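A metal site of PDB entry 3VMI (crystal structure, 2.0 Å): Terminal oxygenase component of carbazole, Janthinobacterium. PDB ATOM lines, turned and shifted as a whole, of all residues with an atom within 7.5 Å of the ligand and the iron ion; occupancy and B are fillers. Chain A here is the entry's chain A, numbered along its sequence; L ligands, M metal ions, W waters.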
ATOM      1  N   ASN A 177      -1.406  -8.100  -1.487  1.00  0.00           N
ATOM      2  CA  ASN A 177      -2.050  -6.929  -2.091  1.00  0.00           C
ATOM      3  C   ASN A 177      -2.240  -7.140  -3.588  1.00  0.00           C
ATOM      4  O   ASN A 177      -3.311  -6.857  -4.132  1.00  0.00           O
ATOM      5  CB  ASN A 177      -1.210  -5.670  -1.865  1.00  0.00           C
ATOM      6  CG  ASN A 177      -1.790  -4.473  -2.576  1.00  0.00           C
ATOM      7  OD1 ASN A 177      -2.805  -3.921  -2.167  1.00  0.00           O
ATOM      8  ND2 ASN A 177      -1.164  -4.082  -3.673  1.00  0.00           N
ATOM      9  N   GLY A 178      -1.210  -7.642  -4.252  1.00  0.00           N
ATOM     10  CA  GLY A 178      -1.290  -7.855  -5.695  1.00  0.00           C
ATOM     11  C   GLY A 178      -2.341  -8.851  -6.141  1.00  0.00           C
ATOM     12  O   GLY A 178      -3.003  -8.650  -7.173  1.00  0.00           O
ATOM     13  N   PHE A 179      -2.507  -9.937  -5.370  1.00  0.00           N
ATOM     14  CA  PHE A 179      -3.470 -10.993  -5.696  1.00  0.00           C
ATOM     15  C   PHE A 179      -4.862 -10.727  -5.098  1.00  0.00           C
ATOM     16  O   PHE A 179      -5.819 -11.457  -5.380  1.00  0.00           O
ATOM     17  CB  PHE A 179      -2.917 -12.341  -5.178  1.00  0.00           C
ATOM     18  CG  PHE A 179      -3.648 -13.540  -5.725  1.00  0.00           C
ATOM     19  CD1 PHE A 179      -3.814 -13.720  -7.090  1.00  0.00           C
ATOM     20  CD2 PHE A 179      -4.170 -14.496  -4.859  1.00  0.00           C
ATOM     21  CE1 PHE A 179      -4.491 -14.827  -7.599  1.00  0.00           C
ATOM     22  CE2 PHE A 179      -4.848 -15.609  -5.354  1.00  0.00           C
ATOM     23  CZ  PHE A 179      -5.002 -15.774  -6.728  1.00  0.00           C
ATOM     24  N   ASP A 180      -4.979  -9.683  -4.284  1.00  0.00           N
ATOM     25  CA  ASP A 180      -6.230  -9.303  -3.608  1.00  0.00           C
ATOM     26  C   ASP A 180      -7.292  -8.860  -4.616  1.00  0.00           C
ATOM     27  O   ASP A 180      -7.177  -7.776  -5.198  1.00  0.00           O
ATOM     28  CB  ASP A 180      -5.917  -8.164  -2.629  1.00  0.00           C
ATOM     29  CG  ASP A 180      -7.054  -7.862  -1.682  1.00  0.00           C
ATOM     30  OD1 ASP A 180      -8.239  -7.917  -2.083  1.00  0.00           O
ATOM     31  OD2 ASP A 180      -6.740  -7.534  -0.510  1.00  0.00           O
ATOM     32  N   HIS A 183      -8.832  -5.306  -3.800  1.00  0.00           N
ATOM     33  CA  HIS A 183      -7.974  -4.132  -3.641  1.00  0.00           C
ATOM     34  C   HIS A 183      -8.077  -3.224  -4.871  1.00  0.00           C
ATOM     35  O   HIS A 183      -7.575  -2.106  -4.876  1.00  0.00           O
ATOM     36  CB  HIS A 183      -6.506  -4.531  -3.400  1.00  0.00           C
ATOM     37  CG  HIS A 183      -5.670  -4.588  -4.629  1.00  0.00           C
ATOM     38  ND1 HIS A 183      -5.770  -5.610  -5.546  1.00  0.00           N
ATOM     39  CD2 HIS A 183      -4.732  -3.741  -5.111  1.00  0.00           C
ATOM     40  CE1 HIS A 183      -4.924  -5.390  -6.544  1.00  0.00           C
ATOM     41  NE2 HIS A 183      -4.277  -4.258  -6.298  1.00  0.00           N
ATOM     42  N   ILE A 184      -8.727  -3.737  -5.914  1.00  0.00           N
ATOM     43  CA  ILE A 184      -8.936  -2.992  -7.155  1.00  0.00           C
ATOM     44  C   ILE A 184      -9.555  -1.622  -6.847  1.00  0.00           C
ATOM     45  O   ILE A 184      -9.434  -0.673  -7.620  1.00  0.00           O
ATOM     46  CB  ILE A 184      -9.854  -3.797  -8.102  1.00  0.00           C
ATOM     47  CG1 ILE A 184      -9.851  -3.196  -9.496  1.00  0.00           C
ATOM     48  CG2 ILE A 184     -11.269  -3.858  -7.550  1.00  0.00           C
ATOM     49  CD1 ILE A 184     -10.664  -4.030 -10.486  1.00  0.00           C
ATOM     50  N   ILE A 186      -8.569   0.567  -4.741  1.00  0.00           N
ATOM     51  CA  ILE A 186      -7.568   1.625  -4.598  1.00  0.00           C
ATOM     52  C   ILE A 186      -7.106   2.203  -5.930  1.00  0.00           C
ATOM     53  O   ILE A 186      -6.451   3.233  -5.961  1.00  0.00           O
ATOM     54  CB  ILE A 186      -6.287   1.154  -3.854  1.00  0.00           C
ATOM     55  CG1 ILE A 186      -5.446   0.264  -4.775  1.00  0.00           C
ATOM     56  CG2 ILE A 186      -6.666   0.431  -2.570  1.00  0.00           C
ATOM     57  CD1 ILE A 186      -4.071  -0.107  -4.189  1.00  0.00           C
ATOM     58  N   HIS A 187      -7.438   1.521  -7.019  1.00  0.00           N
ATOM     59  CA  HIS A 187      -7.043   1.954  -8.352  1.00  0.00           C
ATOM     60  C   HIS A 187      -8.125   2.718  -9.096  1.00  0.00           C
ATOM     61  O   HIS A 187      -7.938   3.083 -10.259  1.00  0.00           O
ATOM     62  CB  HIS A 187      -6.650   0.745  -9.213  1.00  0.00           C
ATOM     63  CG  HIS A 187      -5.434   0.019  -8.743  1.00  0.00           C
ATOM     64  ND1 HIS A 187      -4.211   0.637  -8.602  1.00  0.00           N
ATOM     65  CD2 HIS A 187      -5.250  -1.272  -8.388  1.00  0.00           C
ATOM     66  CE1 HIS A 187      -3.319  -0.244  -8.174  1.00  0.00           C
ATOM     67  NE2 HIS A 187      -3.926  -1.408  -8.036  1.00  0.00           N
ATOM     68  N   ILE A 262      -5.780 -13.500 -13.555  1.00  0.00           N
ATOM     69  CA  ILE A 262      -4.754 -13.088 -12.600  1.00  0.00           C
ATOM     70  C   ILE A 262      -4.336 -14.319 -11.819  1.00  0.00           C
ATOM     71  O   ILE A 262      -5.177 -15.068 -11.324  1.00  0.00           O
ATOM     72  CB  ILE A 262      -5.331 -12.032 -11.629  1.00  0.00           C
ATOM     73  CG1 ILE A 262      -5.935 -10.868 -12.425  1.00  0.00           C
ATOM     74  CG2 ILE A 262      -4.240 -11.512 -10.690  1.00  0.00           C
ATOM     75  CD1 ILE A 262      -6.775  -9.926 -11.605  1.00  0.00           C
ATOM     76  N   LEU A 270       3.323 -12.387  -9.512  1.00  0.00           N
ATOM     77  CA  LEU A 270       1.968 -12.211 -10.013  1.00  0.00           C
ATOM     78  C   LEU A 270       1.948 -12.024 -11.521  1.00  0.00           C
ATOM     79  O   LEU A 270       2.804 -11.324 -12.075  1.00  0.00           O
ATOM     80  CB  LEU A 270       1.323 -10.994  -9.348  1.00  0.00           C
ATOM     81  CG  LEU A 270      -0.161 -10.715  -9.644  1.00  0.00           C
ATOM     82  CD1 LEU A 270      -1.039 -11.598  -8.754  1.00  0.00           C
ATOM     83  CD2 LEU A 270      -0.461  -9.250  -9.374  1.00  0.00           C
ATOM     84  N   VAL A 272      -0.662 -10.841 -14.542  1.00  0.00           N
ATOM     85  CA  VAL A 272      -1.953 -10.228 -14.852  1.00  0.00           C
ATOM     86  C   VAL A 272      -2.027 -10.180 -16.380  1.00  0.00           C
ATOM     87  O   VAL A 272      -1.179  -9.549 -17.035  1.00  0.00           O
ATOM     88  CB  VAL A 272      -2.048  -8.803 -14.264  1.00  0.00           C
ATOM     89  CG1 VAL A 272      -3.460  -8.259 -14.452  1.00  0.00           C
ATOM     90  CG2 VAL A 272      -1.674  -8.823 -12.790  1.00  0.00           C
ATOM     91  N   PHE A 275      -2.658  -6.929 -19.508  1.00  0.00           N
ATOM     92  CA  PHE A 275      -2.507  -5.694 -18.742  1.00  0.00           C
ATOM     93  C   PHE A 275      -1.187  -5.045 -19.106  1.00  0.00           C
ATOM     94  O   PHE A 275      -0.192  -5.745 -19.310  1.00  0.00           O
ATOM     95  CB  PHE A 275      -2.497  -6.017 -17.232  1.00  0.00           C
ATOM     96  CG  PHE A 275      -2.797  -4.839 -16.360  1.00  0.00           C
ATOM     97  CD1 PHE A 275      -4.114  -4.442 -16.132  1.00  0.00           C
ATOM     98  CD2 PHE A 275      -1.762  -4.095 -15.801  1.00  0.00           C
ATOM     99  CE1 PHE A 275      -4.394  -3.324 -15.355  1.00  0.00           C
ATOM    100  CE2 PHE A 275      -2.037  -2.976 -15.015  1.00  0.00           C
ATOM    101  CZ  PHE A 275      -3.352  -2.587 -14.798  1.00  0.00           C
ATOM    102  N   GLN A 282       1.501  -8.450 -17.654  1.00  0.00           N
ATOM    103  CA  GLN A 282       2.338  -7.933 -16.576  1.00  0.00           C
ATOM    104  C   GLN A 282       2.737  -9.100 -15.667  1.00  0.00           C
ATOM    105  O   GLN A 282       1.889  -9.903 -15.275  1.00  0.00           O
ATOM    106  CB  GLN A 282       1.597  -6.873 -15.757  1.00  0.00           C
ATOM    107  CG  GLN A 282       2.469  -6.220 -14.694  1.00  0.00           C
ATOM    108  CD  GLN A 282       1.966  -4.854 -14.277  1.00  0.00           C
ATOM    109  OE1 GLN A 282       1.282  -4.181 -15.042  1.00  0.00           O
ATOM    110  NE2 GLN A 282       2.323  -4.428 -13.073  1.00  0.00           N
ATOM    111  N   GLU A 284       4.996  -9.504 -12.195  1.00  0.00           N
ATOM    112  CA  GLU A 284       5.722  -8.762 -11.168  1.00  0.00           C
ATOM    113  C   GLU A 284       6.068  -9.611  -9.953  1.00  0.00           C
ATOM    114  O   GLU A 284       5.234 -10.341  -9.418  1.00  0.00           O
ATOM    115  CB  GLU A 284       4.950  -7.520 -10.736  1.00  0.00           C
ATOM    116  CG  GLU A 284       3.515  -7.764 -10.274  1.00  0.00           C
ATOM    117  CD  GLU A 284       2.859  -6.470  -9.809  1.00  0.00           C
ATOM    118  OE1 GLU A 284       3.065  -5.450 -10.489  1.00  0.00           O
ATOM    119  OE2 GLU A 284       2.154  -6.475  -8.780  1.00  0.00           O
ATOM    120  N   TYR A 286       7.808  -9.887  -5.974  1.00  0.00           N
ATOM    121  CA  TYR A 286       7.902  -9.179  -4.701  1.00  0.00           C
ATOM    122  C   TYR A 286       9.006 -10.000  -4.019  1.00  0.00           C
ATOM    123  O   TYR A 286       8.736 -10.977  -3.310  1.00  0.00           O
ATOM    124  CB  TYR A 286       6.592  -9.282  -3.925  1.00  0.00           C
ATOM    125  CG  TYR A 286       5.365  -9.028  -4.782  1.00  0.00           C
ATOM    126  CD1 TYR A 286       5.044  -7.738  -5.212  1.00  0.00           C
ATOM    127  CD2 TYR A 286       4.553 -10.081  -5.202  1.00  0.00           C
ATOM    128  CE1 TYR A 286       3.937  -7.503  -6.029  1.00  0.00           C
ATOM    129  CE2 TYR A 286       3.447  -9.854  -6.030  1.00  0.00           C
ATOM    130  CZ  TYR A 286       3.153  -8.575  -6.438  1.00  0.00           C
ATOM    131  OH  TYR A 286       2.056  -8.352  -7.236  1.00  0.00           O
ATOM    132  N   TYR A 296      10.466  -4.672  -5.744  1.00  0.00           N
ATOM    133  CA  TYR A 296       9.208  -4.712  -6.486  1.00  0.00           C
ATOM    134  C   TYR A 296       9.718  -4.737  -7.932  1.00  0.00           C
ATOM    135  O   TYR A 296       9.961  -3.693  -8.544  1.00  0.00           O
ATOM    136  CB  TYR A 296       8.360  -3.476  -6.196  1.00  0.00           C
ATOM    137  CG  TYR A 296       7.062  -3.390  -7.002  1.00  0.00           C
ATOM    138  CD1 TYR A 296       6.380  -4.548  -7.386  1.00  0.00           C
ATOM    139  CD2 TYR A 296       6.527  -2.166  -7.363  1.00  0.00           C
ATOM    140  CE1 TYR A 296       5.185  -4.478  -8.120  1.00  0.00           C
ATOM    141  CE2 TYR A 296       5.338  -2.075  -8.103  1.00  0.00           C
ATOM    142  CZ  TYR A 296       4.677  -3.230  -8.477  1.00  0.00           C
ATOM    143  OH  TYR A 296       3.539  -3.149  -9.255  1.00  0.00           O
ATOM    144  N   PHE A 329      -0.229   3.418 -12.349  1.00  0.00           N
ATOM    145  CA  PHE A 329      -1.195   2.501 -11.785  1.00  0.00           C
ATOM    146  C   PHE A 329      -0.692   1.876 -10.480  1.00  0.00           C
ATOM    147  O   PHE A 329      -1.329   1.998  -9.437  1.00  0.00           O
ATOM    148  CB  PHE A 329      -1.500   1.380 -12.794  1.00  0.00           C
ATOM    149  CG  PHE A 329      -2.654   0.493 -12.395  1.00  0.00           C
ATOM    150  CD1 PHE A 329      -3.966   0.875 -12.661  1.00  0.00           C
ATOM    151  CD2 PHE A 329      -2.414  -0.738 -11.792  1.00  0.00           C
ATOM    152  CE1 PHE A 329      -5.025   0.033 -12.344  1.00  0.00           C
ATOM    153  CE2 PHE A 329      -3.473  -1.595 -11.473  1.00  0.00           C
ATOM    154  CZ  PHE A 329      -4.777  -1.214 -11.754  1.00  0.00           C
ATOM    155  N   ASN A 330       0.465   1.220 -10.550  1.00  0.00           N
ATOM    156  CA  ASN A 330       1.018   0.523  -9.389  1.00  0.00           C
ATOM    157  C   ASN A 330       1.573   1.358  -8.236  1.00  0.00           C
ATOM    158  O   ASN A 330       1.849   0.818  -7.163  1.00  0.00           O
ATOM    159  CB  ASN A 330       2.073  -0.484  -9.871  1.00  0.00           C
ATOM    160  CG  ASN A 330       1.454  -1.594 -10.732  1.00  0.00           C
ATOM    161  OD1 ASN A 330       1.939  -1.878 -11.830  1.00  0.00           O
ATOM    162  ND2 ASN A 330       0.380  -2.204 -10.244  1.00  0.00           N
ATOM    163  N   ASP A 332      -0.006   3.275  -6.354  1.00  0.00           N
ATOM    164  CA  ASP A 332      -0.943   3.179  -5.232  1.00  0.00           C
ATOM    165  C   ASP A 332      -0.782   1.845  -4.502  1.00  0.00           C
ATOM    166  O   ASP A 332      -1.113   1.739  -3.331  1.00  0.00           O
ATOM    167  CB  ASP A 332      -2.395   3.339  -5.701  1.00  0.00           C
ATOM    168  CG  ASP A 332      -2.728   4.775  -6.098  1.00  0.00           C
ATOM    169  OD1 ASP A 332      -2.317   5.698  -5.361  1.00  0.00           O
ATOM    170  OD2 ASP A 332      -3.390   4.976  -7.131  1.00  0.00           O
ATOM    171  N   ASP A 333      -0.274   0.833  -5.190  1.00  0.00           N
ATOM    172  CA  ASP A 333      -0.053  -0.458  -4.545  1.00  0.00           C
ATOM    173  C   ASP A 333       1.060  -0.304  -3.510  1.00  0.00           C
ATOM    174  O   ASP A 333       1.000  -0.901  -2.429  1.00  0.00           O
ATOM    175  CB  ASP A 333       0.350  -1.534  -5.556  1.00  0.00           C
ATOM    176  CG  ASP A 333      -0.781  -1.911  -6.481  1.00  0.00           C
ATOM    177  OD1 ASP A 333      -1.830  -2.362  -5.983  1.00  0.00           O
ATOM    178  OD2 ASP A 333      -0.592  -1.760  -7.708  1.00  0.00           O
ATOM    179  N   ILE A 334       2.046   0.520  -3.842  1.00  0.00           N
ATOM    180  CA  ILE A 334       3.186   0.742  -2.969  1.00  0.00           C
ATOM    181  C   ILE A 334       2.788   1.284  -1.588  1.00  0.00           C
ATOM    182  O   ILE A 334       3.181   0.714  -0.563  1.00  0.00           O
ATOM    183  CB  ILE A 334       4.236   1.695  -3.619  1.00  0.00           C
ATOM    184  CG1 ILE A 334       4.877   1.000  -4.813  1.00  0.00           C
ATOM    185  CG2 ILE A 334       5.303   2.080  -2.602  1.00  0.00           C
ATOM    186  CD1 ILE A 334       5.789   1.897  -5.655  1.00  0.00           C
ATOM    187  N   ALA A 336      -0.137   1.200  -0.287  1.00  0.00           N
ATOM    188  CA  ALA A 336      -1.121   0.309   0.318  1.00  0.00           C
ATOM    189  C   ALA A 336      -0.360  -0.782   1.076  1.00  0.00           C
ATOM    190  O   ALA A 336      -0.750  -1.155   2.179  1.00  0.00           O
ATOM    191  CB  ALA A 336      -2.012  -0.317  -0.750  1.00  0.00           C
ATOM    192  N   ARG A 337       0.714  -1.282   0.478  1.00  0.00           N
ATOM    193  CA  ARG A 337       1.538  -2.312   1.113  1.00  0.00           C
ATOM    194  C   ARG A 337       2.117  -1.754   2.395  1.00  0.00           C
ATOM    195  O   ARG A 337       2.113  -2.425   3.433  1.00  0.00           O
ATOM    196  CB  ARG A 337       2.700  -2.736   0.216  1.00  0.00           C
ATOM    197  CG  ARG A 337       2.302  -3.341  -1.101  1.00  0.00           C
ATOM    198  CD  ARG A 337       3.542  -3.599  -1.949  1.00  0.00           C
ATOM    199  NE  ARG A 337       3.195  -3.691  -3.354  1.00  0.00           N
ATOM    200  CZ  ARG A 337       4.055  -3.599  -4.353  1.00  0.00           C
ATOM    201  NH1 ARG A 337       5.351  -3.423  -4.122  1.00  0.00           N
ATOM    202  NH2 ARG A 337       3.608  -3.685  -5.601  1.00  0.00           N
HETATM  203  O1  LIG L   1      -3.097  -4.607  -9.386  1.00  0.00           O
HETATM  204  O2  LIG L   1      -1.979  -4.200  -8.573  1.00  0.00           O
HETATM  205 FE    FE M   1      -2.963  -3.107  -7.372  1.00  0.00          FE
HETATM  206  O   HOH W   1       1.007  -4.612  -7.093  1.00  0.00           O
HETATM  207  O   HOH W   2      -5.073  -6.867 -10.998  1.00  0.00           O
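Water W1 lies within hydrogen-bond range of OE2 of Glu 284, NH2 of Arg 337 and OD2 of Asp 333.
Residues that only touch the ligand: Asn 330 (3.5 Å) and Phe 329 (3.7 Å).
Hydrophobic or aromatic side chains that line the ligand: His 183 and Phe 329.
Within 4 Å of the ligand: His 183, His 187, Phe 329, Asn 330 and Asp 333.
OD2 of Asp 333 is in hydrogen-bond range of ND2 of Asn 330, 2.8 Å away.
The side-chain amide nitrogen (ND2) of Asn 177 sits close to the side-chain carboxylate (OD1) of Asp 333, 3.0 Å away.
A ring nitrogen (ND1) of His 183 lies within hydrogen-bond range of the backbone carbonyl oxygen of Asn 177 (3.1 Å).
A ring nitrogen (ND1) of His 183 sits at hydrogen-bond distance from the backbone carbonyl oxygen of Asp 180, at 2.6 Å.
The backbone carbonyl oxygen of Phe 329 lies close to a ring nitrogen (ND1) of His 187 (3.3 Å).
OD1 of Asn 330 lies close to OH of Tyr 296 (3.3 Å).
The side-chain amide nitrogen (NE2) of Gln 282 lies within hydrogen-bond range of the side-chain amide oxygen (OD1) of Asn 330, 2.9 Å away.
The iron ion is bound by O2 of the ligand (1.9 Å).
OD1 of Asp 333 binds the iron ion.
The iron ion is bound by NE2 of His 183.
NE2 of His 187 binds the iron ion, at 2.1 Å.
Slightly farther from the iron ion lies the side-chain carboxylate (OD2) of Asp 333 (2.7 Å).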
